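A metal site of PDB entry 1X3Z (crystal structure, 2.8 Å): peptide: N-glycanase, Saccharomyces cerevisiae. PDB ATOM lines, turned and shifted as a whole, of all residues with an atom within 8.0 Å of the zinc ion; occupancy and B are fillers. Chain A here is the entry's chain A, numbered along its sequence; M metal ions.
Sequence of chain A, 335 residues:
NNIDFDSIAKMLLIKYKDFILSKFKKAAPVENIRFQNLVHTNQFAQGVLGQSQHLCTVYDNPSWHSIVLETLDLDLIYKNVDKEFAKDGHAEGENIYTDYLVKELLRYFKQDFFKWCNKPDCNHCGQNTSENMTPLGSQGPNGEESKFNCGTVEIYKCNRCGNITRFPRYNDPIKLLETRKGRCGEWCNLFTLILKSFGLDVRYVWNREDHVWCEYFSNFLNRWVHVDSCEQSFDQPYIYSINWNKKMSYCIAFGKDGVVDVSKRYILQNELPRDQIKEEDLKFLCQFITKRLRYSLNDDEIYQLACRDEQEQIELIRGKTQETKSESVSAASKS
The zinc ion is bound by the side-chain sulfur of Cys 125 (2.1 Å), the side-chain sulfur of Cys 158 (2.3 Å), the side-chain sulfur of Cys 161 (2.3 Å) and the side-chain sulfur of Cys 122 (2.3 Å). The zinc ion has four donor atoms within binding distance.
O of Asn 132 lies close to SG of Cys 158 (3.4 Å). The backbone carbonyl oxygen (O) of Asn 163 lies within hydrogen-bond range of the backbone NH (N) of Cys 158 (3.0 Å). The backbone NH of Cys 122 lies within hydrogen-bond range of the backbone carbonyl oxygen of Thr 129. SG of Cys 158 sits close to N of Arg 160 (3.4 Å). The backbone NH of Asn 163 sits close to the side-chain sulfur of Cys 161, at 3.3 Å.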
ATOM      1  N   ASP A 121     -14.202 -21.630 -15.919  1.00  0.00           N
ATOM      2  CA  ASP A 121     -14.741 -22.213 -14.715  1.00  0.00           C
ATOM      3  C   ASP A 121     -16.168 -22.503 -14.997  1.00  0.00           C
ATOM      4  O   ASP A 121     -16.746 -21.924 -15.907  1.00  0.00           O
ATOM      5  CB  ASP A 121     -14.589 -21.293 -13.529  1.00  0.00           C
ATOM      6  CG  ASP A 121     -13.126 -21.163 -13.093  1.00  0.00           C
ATOM      7  OD1 ASP A 121     -12.268 -21.926 -13.616  1.00  0.00           O
ATOM      8  OD2 ASP A 121     -12.820 -20.316 -12.226  1.00  0.00           O
ATOM      9  N   CYS A 122     -16.720 -23.429 -14.233  1.00  0.00           N
ATOM     10  CA  CYS A 122     -18.060 -23.885 -14.525  1.00  0.00           C
ATOM     11  C   CYS A 122     -19.022 -22.934 -13.870  1.00  0.00           C
ATOM     12  O   CYS A 122     -19.051 -22.796 -12.652  1.00  0.00           O
ATOM     13  CB  CYS A 122     -18.283 -25.302 -14.008  1.00  0.00           C
ATOM     14  SG  CYS A 122     -19.938 -25.910 -14.321  1.00  0.00           S
ATOM     15  N   ASN A 123     -19.786 -22.228 -14.694  1.00  0.00           N
ATOM     16  CA  ASN A 123     -20.589 -21.175 -14.123  1.00  0.00           C
ATOM     17  C   ASN A 123     -21.704 -21.691 -13.239  1.00  0.00           C
ATOM     18  O   ASN A 123     -22.003 -21.057 -12.241  1.00  0.00           O
ATOM     19  CB  ASN A 123     -21.046 -20.122 -15.146  1.00  0.00           C
ATOM     20  CG  ASN A 123     -21.601 -20.712 -16.420  1.00  0.00           C
ATOM     21  OD1 ASN A 123     -21.107 -20.429 -17.509  1.00  0.00           O
ATOM     22  ND2 ASN A 123     -22.660 -21.525 -16.298  1.00  0.00           N
ATOM     23  N   HIS A 124     -22.284 -22.847 -13.547  1.00  0.00           N
ATOM     24  CA  HIS A 124     -23.235 -23.400 -12.594  1.00  0.00           C
ATOM     25  C   HIS A 124     -22.565 -23.803 -11.266  1.00  0.00           C
ATOM     26  O   HIS A 124     -23.027 -23.422 -10.195  1.00  0.00           O
ATOM     27  CB  HIS A 124     -24.048 -24.571 -13.124  1.00  0.00           C
ATOM     28  CG  HIS A 124     -24.759 -25.305 -12.034  1.00  0.00           C
ATOM     29  ND1 HIS A 124     -26.018 -24.934 -11.589  1.00  0.00           N
ATOM     30  CD2 HIS A 124     -24.357 -26.316 -11.217  1.00  0.00           C
ATOM     31  CE1 HIS A 124     -26.373 -25.717 -10.589  1.00  0.00           C
ATOM     32  NE2 HIS A 124     -25.389 -26.557 -10.343  1.00  0.00           N
ATOM     33  N   CYS A 125     -21.493 -24.598 -11.330  1.00  0.00           N
ATOM     34  CA  CYS A 125     -20.804 -25.082 -10.126  1.00  0.00           C
ATOM     35  C   CYS A 125     -20.191 -23.924  -9.370  1.00  0.00           C
ATOM     36  O   CYS A 125     -20.503 -22.784  -9.661  1.00  0.00           O
ATOM     37  CB  CYS A 125     -19.688 -26.066 -10.481  1.00  0.00           C
ATOM     38  SG  CYS A 125     -20.280 -27.590 -11.150  1.00  0.00           S
ATOM     39  N   GLY A 126     -19.305 -24.222  -8.421  1.00  0.00           N
ATOM     40  CA  GLY A 126     -18.507 -23.203  -7.732  1.00  0.00           C
ATOM     41  C   GLY A 126     -17.691 -22.295  -8.666  1.00  0.00           C
ATOM     42  O   GLY A 126     -17.921 -22.213  -9.881  1.00  0.00           O
ATOM     43  N   THR A 129     -13.342 -24.153 -10.344  1.00  0.00           N
ATOM     44  CA  THR A 129     -13.627 -25.439 -10.947  1.00  0.00           C
ATOM     45  C   THR A 129     -13.253 -25.485 -12.440  1.00  0.00           C
ATOM     46  O   THR A 129     -13.981 -24.947 -13.270  1.00  0.00           O
ATOM     47  CB  THR A 129     -15.139 -25.654 -10.900  1.00  0.00           C
ATOM     48  OG1 THR A 129     -15.570 -26.303 -12.102  1.00  0.00           O
ATOM     49  CG2 THR A 129     -15.848 -24.303 -10.822  1.00  0.00           C
ATOM     50  N   ASN A 132     -12.844 -30.739 -14.170  1.00  0.00           N
ATOM     51  CA  ASN A 132     -14.151 -31.279 -14.383  1.00  0.00           C
ATOM     52  C   ASN A 132     -14.806 -30.410 -15.474  1.00  0.00           C
ATOM     53  O   ASN A 132     -16.000 -30.110 -15.441  1.00  0.00           O
ATOM     54  CB  ASN A 132     -14.927 -31.228 -13.062  1.00  0.00           C
ATOM     55  CG  ASN A 132     -14.578 -29.995 -12.233  1.00  0.00           C
ATOM     56  OD1 ASN A 132     -13.431 -29.527 -12.247  1.00  0.00           O
ATOM     57  ND2 ASN A 132     -15.557 -29.473 -11.490  1.00  0.00           N
ATOM     58  N   MET A 133     -13.963 -29.983 -16.409  1.00  0.00           N
ATOM     59  CA  MET A 133     -14.401 -29.356 -17.641  1.00  0.00           C
ATOM     60  C   MET A 133     -13.708 -30.126 -18.761  1.00  0.00           C
ATOM     61  O   MET A 133     -12.489 -30.184 -18.814  1.00  0.00           O
ATOM     62  CB  MET A 133     -14.005 -27.876 -17.637  1.00  0.00           C
ATOM     63  CG  MET A 133     -14.583 -27.075 -16.470  1.00  0.00           C
ATOM     64  SD  MET A 133     -16.372 -27.059 -16.441  1.00  0.00           S
ATOM     65  CE  MET A 133     -16.760 -26.486 -18.045  1.00  0.00           C
ATOM     66  N   LYS A 157     -17.816 -28.846 -21.348  1.00  0.00           N
ATOM     67  CA  LYS A 157     -18.795 -29.618 -20.597  1.00  0.00           C
ATOM     68  C   LYS A 157     -18.235 -29.856 -19.240  1.00  0.00           C
ATOM     69  O   LYS A 157     -17.087 -30.259 -19.125  1.00  0.00           O
ATOM     70  CB  LYS A 157     -19.050 -30.947 -21.270  1.00  0.00           C
ATOM     71  CG  LYS A 157     -20.070 -31.808 -20.571  1.00  0.00           C
ATOM     72  CD  LYS A 157     -21.469 -31.262 -20.727  1.00  0.00           C
ATOM     73  CE  LYS A 157     -22.505 -32.358 -20.562  1.00  0.00           C
ATOM     74  NZ  LYS A 157     -23.799 -31.988 -21.183  1.00  0.00           N
ATOM     75  N   CYS A 158     -19.048 -29.585 -18.231  1.00  0.00           N
ATOM     76  CA  CYS A 158     -18.662 -29.791 -16.864  1.00  0.00           C
ATOM     77  C   CYS A 158     -19.009 -31.195 -16.483  1.00  0.00           C
ATOM     78  O   CYS A 158     -20.098 -31.651 -16.764  1.00  0.00           O
ATOM     79  CB  CYS A 158     -19.387 -28.840 -15.927  1.00  0.00           C
ATOM     80  SG  CYS A 158     -19.007 -29.132 -14.172  1.00  0.00           S
ATOM     81  N   ASN A 159     -18.073 -31.863 -15.827  1.00  0.00           N
ATOM     82  CA  ASN A 159     -18.234 -33.266 -15.483  1.00  0.00           C
ATOM     83  C   ASN A 159     -18.826 -33.492 -14.109  1.00  0.00           C
ATOM     84  O   ASN A 159     -18.859 -34.618 -13.648  1.00  0.00           O
ATOM     85  CB  ASN A 159     -16.902 -33.965 -15.629  1.00  0.00           C
ATOM     86  CG  ASN A 159     -16.627 -34.361 -17.048  1.00  0.00           C
ATOM     87  OD1 ASN A 159     -17.550 -34.670 -17.792  1.00  0.00           O
ATOM     88  ND2 ASN A 159     -15.375 -34.333 -17.454  1.00  0.00           N
ATOM     89  N   ARG A 160     -19.313 -32.441 -13.478  1.00  0.00           N
ATOM     90  CA  ARG A 160     -19.709 -32.549 -12.091  1.00  0.00           C
ATOM     91  C   ARG A 160     -21.182 -32.208 -11.938  1.00  0.00           C
ATOM     92  O   ARG A 160     -21.828 -32.620 -10.968  1.00  0.00           O
ATOM     93  CB  ARG A 160     -18.845 -31.596 -11.277  1.00  0.00           C
ATOM     94  CG  ARG A 160     -18.192 -32.201 -10.087  1.00  0.00           C
ATOM     95  CD  ARG A 160     -16.957 -32.997 -10.474  1.00  0.00           C
ATOM     96  NE  ARG A 160     -16.278 -33.599  -9.320  1.00  0.00           N
ATOM     97  CZ  ARG A 160     -15.389 -32.983  -8.538  1.00  0.00           C
ATOM     98  NH1 ARG A 160     -15.050 -31.702  -8.747  1.00  0.00           N
ATOM     99  NH2 ARG A 160     -14.832 -33.640  -7.525  1.00  0.00           N
ATOM    100  N   CYS A 161     -21.709 -31.443 -12.899  1.00  0.00           N
ATOM    101  CA  CYS A 161     -23.102 -31.027 -12.913  1.00  0.00           C
ATOM    102  C   CYS A 161     -23.612 -31.245 -14.317  1.00  0.00           C
ATOM    103  O   CYS A 161     -24.820 -31.175 -14.585  1.00  0.00           O
ATOM    104  CB  CYS A 161     -23.211 -29.548 -12.588  1.00  0.00           C
ATOM    105  SG  CYS A 161     -22.630 -28.452 -13.932  1.00  0.00           S
ATOM    106  N   GLY A 162     -22.671 -31.477 -15.225  1.00  0.00           N
ATOM    107  CA  GLY A 162     -22.967 -31.808 -16.610  1.00  0.00           C
ATOM    108  C   GLY A 162     -23.576 -30.685 -17.414  1.00  0.00           C
ATOM    109  O   GLY A 162     -24.340 -30.937 -18.317  1.00  0.00           O
ATOM    110  N   ASN A 163     -23.216 -29.460 -17.069  1.00  0.00           N
ATOM    111  CA  ASN A 163     -23.666 -28.257 -17.787  1.00  0.00           C
ATOM    112  C   ASN A 163     -22.613 -27.699 -18.746  1.00  0.00           C
ATOM    113  O   ASN A 163     -21.407 -27.780 -18.459  1.00  0.00           O
ATOM    114  CB  ASN A 163     -24.031 -27.165 -16.784  1.00  0.00           C
ATOM    115  CG  ASN A 163     -25.485 -27.145 -16.460  1.00  0.00           C
ATOM    116  OD1 ASN A 163     -25.869 -27.149 -15.276  1.00  0.00           O
ATOM    117  ND2 ASN A 163     -26.343 -27.091 -17.494  1.00  0.00           N
ATOM    118  N   ILE A 164     -23.085 -27.132 -19.856  1.00  0.00           N
ATOM    119  CA  ILE A 164     -22.191 -26.433 -20.785  1.00  0.00           C
ATOM    120  C   ILE A 164     -21.783 -25.090 -20.212  1.00  0.00           C
ATOM    121  O   ILE A 164     -22.617 -24.365 -19.709  1.00  0.00           O
ATOM    122  CB  ILE A 164     -22.874 -26.169 -22.135  1.00  0.00           C
ATOM    123  CG1 ILE A 164     -23.357 -27.481 -22.765  1.00  0.00           C
ATOM    124  CG2 ILE A 164     -21.955 -25.379 -23.054  1.00  0.00           C
ATOM    125  CD1 ILE A 164     -22.254 -28.319 -23.373  1.00  0.00           C
ATOM    126  N   THR A 165     -20.501 -24.762 -20.301  1.00  0.00           N
ATOM    127  CA  THR A 165     -20.044 -23.407 -20.035  1.00  0.00           C
ATOM    128  C   THR A 165     -19.340 -22.972 -21.309  1.00  0.00           C
ATOM    129  O   THR A 165     -18.686 -23.805 -21.954  1.00  0.00           O
ATOM    130  CB  THR A 165     -19.092 -23.370 -18.811  1.00  0.00           C
ATOM    131  OG1 THR A 165     -19.841 -23.630 -17.620  1.00  0.00           O
ATOM    132  CG2 THR A 165     -18.355 -22.014 -18.682  1.00  0.00           C
HETATM  133 ZN    ZN M   1     -20.580 -27.813 -13.245  1.00  0.00          ZN
